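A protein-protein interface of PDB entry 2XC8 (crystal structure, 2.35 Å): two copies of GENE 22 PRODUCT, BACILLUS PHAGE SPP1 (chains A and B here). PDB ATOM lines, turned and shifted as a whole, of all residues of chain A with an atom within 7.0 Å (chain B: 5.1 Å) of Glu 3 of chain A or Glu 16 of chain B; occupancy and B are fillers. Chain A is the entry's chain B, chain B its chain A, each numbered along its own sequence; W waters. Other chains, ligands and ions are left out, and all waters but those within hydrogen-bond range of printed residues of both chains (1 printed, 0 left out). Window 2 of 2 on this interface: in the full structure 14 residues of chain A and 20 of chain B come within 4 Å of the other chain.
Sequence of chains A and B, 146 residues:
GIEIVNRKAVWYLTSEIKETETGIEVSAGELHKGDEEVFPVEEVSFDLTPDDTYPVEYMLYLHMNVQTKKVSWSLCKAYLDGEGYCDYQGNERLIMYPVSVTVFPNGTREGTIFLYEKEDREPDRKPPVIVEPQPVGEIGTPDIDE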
ATOM      1  N   GLY A   1      22.108  32.380 -10.771  1.00  0.00           N
ATOM      2  CA  GLY A   1      21.220  32.137 -11.956  1.00  0.00           C
ATOM      3  C   GLY A   1      21.189  30.680 -12.370  1.00  0.00           C
ATOM      4  O   GLY A   1      21.388  29.785 -11.545  1.00  0.00           O
ATOM      5  N   ILE A   2      20.931  30.440 -13.654  1.00  0.00           N
ATOM      6  CA  ILE A   2      20.977  29.087 -14.200  1.00  0.00           C
ATOM      7  C   ILE A   2      22.344  28.821 -14.833  1.00  0.00           C
ATOM      8  O   ILE A   2      22.670  29.332 -15.908  1.00  0.00           O
ATOM      9  CB  ILE A   2      19.811  28.795 -15.181  1.00  0.00           C
ATOM     10  CG1 ILE A   2      18.464  29.014 -14.481  1.00  0.00           C
ATOM     11  CG2 ILE A   2      19.905  27.365 -15.707  1.00  0.00           C
ATOM     12  CD1 ILE A   2      17.263  29.033 -15.408  1.00  0.00           C
ATOM     13  N   GLU A   3      23.132  28.017 -14.124  1.00  0.00           N
ATOM     14  CA  GLU A   3      24.498  27.679 -14.504  1.00  0.00           C
ATOM     15  C   GLU A   3      24.509  26.655 -15.636  1.00  0.00           C
ATOM     16  O   GLU A   3      23.545  25.907 -15.815  1.00  0.00           O
ATOM     17  CB  GLU A   3      25.236  27.115 -13.286  1.00  0.00           C
ATOM     18  CG  GLU A   3      26.758  27.194 -13.361  1.00  0.00           C
ATOM     19  CD  GLU A   3      27.453  26.263 -12.376  1.00  0.00           C
ATOM     20  OE1 GLU A   3      26.769  25.452 -11.713  1.00  0.00           O
ATOM     21  OE2 GLU A   3      28.695  26.339 -12.268  1.00  0.00           O
ATOM     22  N   ILE A   4      25.598  26.629 -16.399  1.00  0.00           N
ATOM     23  CA  ILE A   4      25.770  25.629 -17.447  1.00  0.00           C
ATOM     24  C   ILE A   4      26.922  24.683 -17.111  1.00  0.00           C
ATOM     25  O   ILE A   4      28.030  25.125 -16.779  1.00  0.00           O
ATOM     26  CB  ILE A   4      25.925  26.278 -18.847  1.00  0.00           C
ATOM     27  CG1 ILE A   4      24.568  26.845 -19.289  1.00  0.00           C
ATOM     28  CG2 ILE A   4      26.472  25.273 -19.866  1.00  0.00           C
ATOM     29  CD1 ILE A   4      24.549  27.498 -20.662  1.00  0.00           C
ATOM     30  N   VAL A   5      26.638  23.383 -17.181  1.00  0.00           N
ATOM     31  CA  VAL A   5      27.633  22.353 -16.893  1.00  0.00           C
ATOM     32  C   VAL A   5      27.881  21.469 -18.118  1.00  0.00           C
ATOM     33  O   VAL A   5      27.026  20.673 -18.518  1.00  0.00           O
ATOM     34  CB  VAL A   5      27.257  21.508 -15.638  1.00  0.00           C
ATOM     35  CG1 VAL A   5      28.202  20.316 -15.477  1.00  0.00           C
ATOM     36  CG2 VAL A   5      27.305  22.374 -14.383  1.00  0.00           C
ATOM     37  N   ASN A   6      29.060  21.647 -18.713  1.00  0.00           N
ATOM     38  CA  ASN A   6      29.517  20.825 -19.826  1.00  0.00           C
ATOM     39  C   ASN A   6      30.193  19.562 -19.302  1.00  0.00           C
ATOM     40  O   ASN A   6      31.050  19.636 -18.418  1.00  0.00           O
ATOM     41  CB  ASN A   6      30.506  21.605 -20.704  1.00  0.00           C
ATOM     42  CG  ASN A   6      29.882  22.830 -21.354  1.00  0.00           C
ATOM     43  OD1 ASN A   6      30.333  23.956 -21.141  1.00  0.00           O
ATOM     44  ND2 ASN A   6      28.841  22.616 -22.152  1.00  0.00           N
ATOM     45  N   GLU A  19      18.282  29.144 -21.559  1.00  0.00           N
ATOM     46  CA  GLU A  19      17.346  29.903 -20.742  1.00  0.00           C
ATOM     47  C   GLU A  19      16.855  31.118 -21.524  1.00  0.00           C
ATOM     48  O   GLU A  19      17.654  31.883 -22.072  1.00  0.00           O
ATOM     49  CB  GLU A  19      18.014  30.352 -19.438  1.00  0.00           C
ATOM     50  CG  GLU A  19      17.101  31.136 -18.493  1.00  0.00           C
ATOM     51  CD  GLU A  19      17.860  31.914 -17.425  1.00  0.00           C
ATOM     52  OE1 GLU A  19      19.102  31.795 -17.347  1.00  0.00           O
ATOM     53  OE2 GLU A  19      17.204  32.649 -16.656  1.00  0.00           O
ATOM     54  N   PRO A  98      18.768  16.902 -18.071  1.00  0.00           N
ATOM     55  CA  PRO A  98      19.563  18.066 -18.497  1.00  0.00           C
ATOM     56  C   PRO A  98      19.177  19.423 -17.881  1.00  0.00           C
ATOM     57  O   PRO A  98      19.971  20.362 -17.954  1.00  0.00           O
ATOM     58  CB  PRO A  98      19.368  18.087 -20.019  1.00  0.00           C
ATOM     59  CG  PRO A  98      18.055  17.429 -20.241  1.00  0.00           C
ATOM     60  CD  PRO A  98      17.879  16.414 -19.143  1.00  0.00           C
ATOM     61  N   ARG A 109      15.786  32.708 -10.379  1.00  0.00           N
ATOM     62  CA  ARG A 109      16.034  31.345 -10.835  1.00  0.00           C
ATOM     63  C   ARG A 109      17.399  30.858 -10.364  1.00  0.00           C
ATOM     64  O   ARG A 109      18.407  31.540 -10.548  1.00  0.00           O
ATOM     65  CB  ARG A 109      15.951  31.270 -12.362  1.00  0.00           C
ATOM     66  CG  ARG A 109      14.604  31.681 -12.936  1.00  0.00           C
ATOM     67  CD  ARG A 109      14.708  31.981 -14.418  1.00  0.00           C
ATOM     68  NE  ARG A 109      13.424  32.401 -14.975  1.00  0.00           N
ATOM     69  CZ  ARG A 109      13.216  32.705 -16.253  1.00  0.00           C
ATOM     70  NH1 ARG A 109      14.209  32.637 -17.133  1.00  0.00           N
ATOM     71  NH2 ARG A 109      12.009  33.077 -16.656  1.00  0.00           N
ATOM     72  N   GLU A 110      17.416  29.681  -9.745  1.00  0.00           N
ATOM     73  CA  GLU A 110      18.657  29.034  -9.336  1.00  0.00           C
ATOM     74  C   GLU A 110      18.649  27.582  -9.793  1.00  0.00           C
ATOM     75  O   GLU A 110      17.748  26.815  -9.439  1.00  0.00           O
ATOM     76  CB  GLU A 110      18.853  29.134  -7.817  1.00  0.00           C
ATOM     77  CG  GLU A 110      20.120  28.453  -7.274  1.00  0.00           C
ATOM     78  CD  GLU A 110      21.422  29.088  -7.758  1.00  0.00           C
ATOM     79  OE1 GLU A 110      22.472  28.418  -7.659  1.00  0.00           O
ATOM     80  OE2 GLU A 110      21.405  30.248  -8.231  1.00  0.00           O
ATOM     81  N   GLY A 111      19.649  27.210 -10.587  1.00  0.00           N
ATOM     82  CA  GLY A 111      19.739  25.849 -11.099  1.00  0.00           C
ATOM     83  C   GLY A 111      20.838  25.600 -12.110  1.00  0.00           C
ATOM     84  O   GLY A 111      21.817  26.348 -12.184  1.00  0.00           O
ATOM     85  N   THR A 112      20.661  24.539 -12.895  1.00  0.00           N
ATOM     86  CA  THR A 112      21.688  24.067 -13.818  1.00  0.00           C
ATOM     87  C   THR A 112      21.190  23.484 -15.142  1.00  0.00           C
ATOM     88  O   THR A 112      20.180  22.778 -15.187  1.00  0.00           O
ATOM     89  CB  THR A 112      22.537  22.936 -13.178  1.00  0.00           C
ATOM     90  OG1 THR A 112      22.942  23.319 -11.857  1.00  0.00           O
ATOM     91  CG2 THR A 112      23.775  22.641 -14.010  1.00  0.00           C
ATOM     92  N   ILE A 113      21.913  23.806 -16.213  1.00  0.00           N
ATOM     93  CA  ILE A 113      21.605  23.255 -17.528  1.00  0.00           C
ATOM     94  C   ILE A 113      22.799  22.336 -17.790  1.00  0.00           C
ATOM     95  O   ILE A 113      23.945  22.793 -17.853  1.00  0.00           O
ATOM     96  CB  ILE A 113      21.449  24.304 -18.664  1.00  0.00           C
ATOM     97  CG1 ILE A 113      20.103  25.026 -18.548  1.00  0.00           C
ATOM     98  CG2 ILE A 113      21.576  23.645 -20.041  1.00  0.00           C
ATOM     99  CD1 ILE A 113      19.999  26.307 -19.366  1.00  0.00           C
ATOM    100  N   PHE A 114      22.528  21.039 -17.920  1.00  0.00           N
ATOM    101  CA  PHE A 114      23.570  20.053 -18.197  1.00  0.00           C
ATOM    102  C   PHE A 114      23.690  19.816 -19.701  1.00  0.00           C
ATOM    103  O   PHE A 114      22.743  19.353 -20.344  1.00  0.00           O
ATOM    104  CB  PHE A 114      23.281  18.734 -17.467  1.00  0.00           C
ATOM    105  CG  PHE A 114      23.428  18.815 -15.970  1.00  0.00           C
ATOM    106  CD1 PHE A 114      24.657  18.573 -15.363  1.00  0.00           C
ATOM    107  CD2 PHE A 114      22.333  19.116 -15.166  1.00  0.00           C
ATOM    108  CE1 PHE A 114      24.796  18.641 -13.976  1.00  0.00           C
ATOM    109  CE2 PHE A 114      22.460  19.187 -13.779  1.00  0.00           C
ATOM    110  CZ  PHE A 114      23.695  18.950 -13.185  1.00  0.00           C
ATOM    111  N   THR B  14      22.960  36.552 -23.158  1.00  0.00           N
ATOM    112  CA  THR B  14      22.671  35.614 -22.069  1.00  0.00           C
ATOM    113  C   THR B  14      23.565  34.372 -22.114  1.00  0.00           C
ATOM    114  O   THR B  14      23.485  33.509 -21.234  1.00  0.00           O
ATOM    115  CB  THR B  14      21.181  35.194 -22.047  1.00  0.00           C
ATOM    116  OG1 THR B  14      20.825  34.601 -23.303  1.00  0.00           O
ATOM    117  CG2 THR B  14      20.279  36.395 -21.776  1.00  0.00           C
ATOM    118  N   SER B  15      24.412  34.293 -23.142  1.00  0.00           N
ATOM    119  CA  SER B  15      25.386  33.213 -23.278  1.00  0.00           C
ATOM    120  C   SER B  15      26.386  33.221 -22.128  1.00  0.00           C
ATOM    121  O   SER B  15      26.917  34.269 -21.755  1.00  0.00           O
ATOM    122  CB  SER B  15      26.141  33.324 -24.604  1.00  0.00           C
ATOM    123  OG  SER B  15      25.301  33.036 -25.707  1.00  0.00           O
ATOM    124  N   GLU B  16      26.624  32.038 -21.573  1.00  0.00           N
ATOM    125  CA  GLU B  16      27.622  31.840 -20.534  1.00  0.00           C
ATOM    126  C   GLU B  16      29.004  31.764 -21.180  1.00  0.00           C
ATOM    127  O   GLU B  16      29.255  30.894 -22.019  1.00  0.00           O
ATOM    128  CB  GLU B  16      27.312  30.553 -19.765  1.00  0.00           C
ATOM    129  CG  GLU B  16      28.131  30.338 -18.503  1.00  0.00           C
ATOM    130  CD  GLU B  16      27.423  29.431 -17.511  1.00  0.00           C
ATOM    131  OE1 GLU B  16      28.000  28.385 -17.143  1.00  0.00           O
ATOM    132  OE2 GLU B  16      26.286  29.759 -17.103  1.00  0.00           O
ATOM    133  N   ILE B  17      29.888  32.683 -20.799  1.00  0.00           N
ATOM    134  CA  ILE B  17      31.254  32.697 -21.322  1.00  0.00           C
ATOM    135  C   ILE B  17      32.241  32.396 -20.197  1.00  0.00           C
ATOM    136  O   ILE B  17      32.244  33.081 -19.170  1.00  0.00           O
ATOM    137  CB  ILE B  17      31.609  34.048 -21.999  1.00  0.00           C
ATOM    138  CG1 ILE B  17      30.533  34.448 -23.016  1.00  0.00           C
ATOM    139  CG2 ILE B  17      32.983  33.969 -22.668  1.00  0.00           C
ATOM    140  CD1 ILE B  17      30.509  35.931 -23.357  1.00  0.00           C
ATOM    141  N   LYS B  18      33.070  31.373 -20.387  1.00  0.00           N
ATOM    142  CA  LYS B  18      34.039  30.987 -19.362  1.00  0.00           C
ATOM    143  C   LYS B  18      35.405  30.563 -19.901  1.00  0.00           C
ATOM    144  O   LYS B  18      35.527  30.074 -21.029  1.00  0.00           O
ATOM    145  CB  LYS B  18      33.459  29.908 -18.432  1.00  0.00           C
ATOM    146  CG  LYS B  18      33.267  28.531 -19.060  1.00  0.00           C
ATOM    147  CD  LYS B  18      32.718  27.542 -18.037  1.00  0.00           C
ATOM    148  CE  LYS B  18      32.796  26.107 -18.540  1.00  0.00           C
ATOM    149  NZ  LYS B  18      31.859  25.845 -19.686  1.00  0.00           N
ATOM    150  N   GLU B  25      35.142  28.933 -23.682  1.00  0.00           N
ATOM    151  CA  GLU B  25      33.878  28.295 -24.045  1.00  0.00           C
ATOM    152  C   GLU B  25      32.710  29.267 -23.906  1.00  0.00           C
ATOM    153  O   GLU B  25      32.471  29.817 -22.828  1.00  0.00           O
ATOM    154  CB  GLU B  25      33.628  27.050 -23.186  1.00  0.00           C
ATOM    155  CG  GLU B  25      33.987  25.735 -23.872  1.00  0.00           C
ATOM    156  CD  GLU B  25      34.058  24.563 -22.901  1.00  0.00           C
ATOM    157  OE1 GLU B  25      33.194  24.462 -22.000  1.00  0.00           O
ATOM    158  OE2 GLU B  25      34.982  23.734 -23.047  1.00  0.00           O
ATOM    159  N   VAL B  26      31.998  29.481 -25.008  1.00  0.00           N
ATOM    160  CA  VAL B  26      30.791  30.301 -25.009  1.00  0.00           C
ATOM    161  C   VAL B  26      29.597  29.391 -25.268  1.00  0.00           C
ATOM    162  O   VAL B  26      29.555  28.680 -26.274  1.00  0.00           O
ATOM    163  CB  VAL B  26      30.847  31.425 -26.077  1.00  0.00           C
ATOM    164  CG1 VAL B  26      29.595  32.296 -26.016  1.00  0.00           C
ATOM    165  CG2 VAL B  26      32.096  32.281 -25.897  1.00  0.00           C
ATOM    166  N   SER B  27      28.639  29.406 -24.347  1.00  0.00           N
ATOM    167  CA  SER B  27      27.441  28.589 -24.474  1.00  0.00           C
ATOM    168  C   SER B  27      26.472  29.198 -25.482  1.00  0.00           C
ATOM    169  O   SER B  27      26.622  30.355 -25.881  1.00  0.00           O
ATOM    170  CB  SER B  27      26.758  28.435 -23.116  1.00  0.00           C
ATOM    171  OG  SER B  27      26.103  29.632 -22.735  1.00  0.00           O
HETATM  172  O   HOH W   1      20.524  31.817 -22.679  1.00  0.00           O
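Water W1 lies within hydrogen-bond range of the side-chain hydroxyl (OG1) of Thr 14 of chain B and the backbone carbonyl oxygen (O) of Glu 19 of chain A.
The side-chain carboxylate (OE1) of Glu 16 of chain B is in hydrogen-bond range of the backbone NH (N) of Ile 4 of chain A (3.1 Å). NZ of Lys 18 of chain B is in hydrogen-bond range of OD1 of Asn 6 of chain A (2.8 Å). The side-chain carboxylate of Glu 25 of chain B sits close to the side-chain amide oxygen of Asn 6 of chain A (3.0 Å).
Among the printed residues, pairs that only touch across the chains: Ile 4 of chain A with Ser 27 of chain B (3.4 Å), Glu 3 of chain A with Glu 16 of chain B (3.8 Å) and Ile 2 of chain A with Glu 16 of chain B (3.8 Å).
Of chain B, only Glu 16 (3.8 Å) comes within 4 Å of Glu 3 of chain A. Printed residues of chain B within 4 Å of Ile 4 of chain A: Glu 16 and Ser 27. Val 5 of chain A touches none of the printed residues of chain B. Ser 15 of chain B touches none of the printed residues of chain A. Glu 16 of chain B touches three residues of chain A. Of the printed residues of chain A, Lys 18 of chain B touches Asn 6. Printed residues of chain A within 4 Å of Glu 25 of chain B: Asn 6 (3.0 Å). Printed residues of chain A within 4 Å of Ser 27 of chain B: Ile 4. The nearest printed residue of chain B that does not touch Glu 3 of chain A is Lys 18 of chain B (7.1 Å). The nearest printed residue of chain A that does not touch Glu 25 of chain B is Ile 4 of chain A (7.1 Å).
No position is printed for both chains. Of the 6 pairs that touch across the chains among the printed residues, none has its exchanged pair printed and touching as well.
Printed residues of chain A that touch a printed residue of chain B: Ile 2, Glu 3, Ile 4 and Asn 6. Of the 8 printed residues of chain B, 4 touch a printed residue of chain A. Printed residues of chain B that touch a printed residue of chain A: Glu 16, Lys 18, Glu 25 and Ser 27. Among the printed residues, 6 pairs touch across the chains.
The side-chain hydroxyl (OG) of Ser 15 of chain B lies within hydrogen-bond range of the backbone carbonyl oxygen (O) of Ser 27 of chain B, 3.0 Å away. The backbone NH (N) of Glu 16 of chain B lies within hydrogen-bond range of the side-chain hydroxyl (OG) of Ser 27 of chain B. The side-chain carboxylate (OE1) of Glu 25 of chain B lies within salt-bridge range of the side-chain amino group (NZ) of Lys 18 of chain B, at 3.0 Å. The backbone NH (N) of Glu 3 of chain A is in hydrogen-bond range of the backbone carbonyl oxygen (O) of Gly 111 of chain A. The backbone carbonyl oxygen (O) of Glu 3 of chain A is in hydrogen-bond range of the backbone NH (N) of Ile 113 of chain A, 2.7 Å away.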
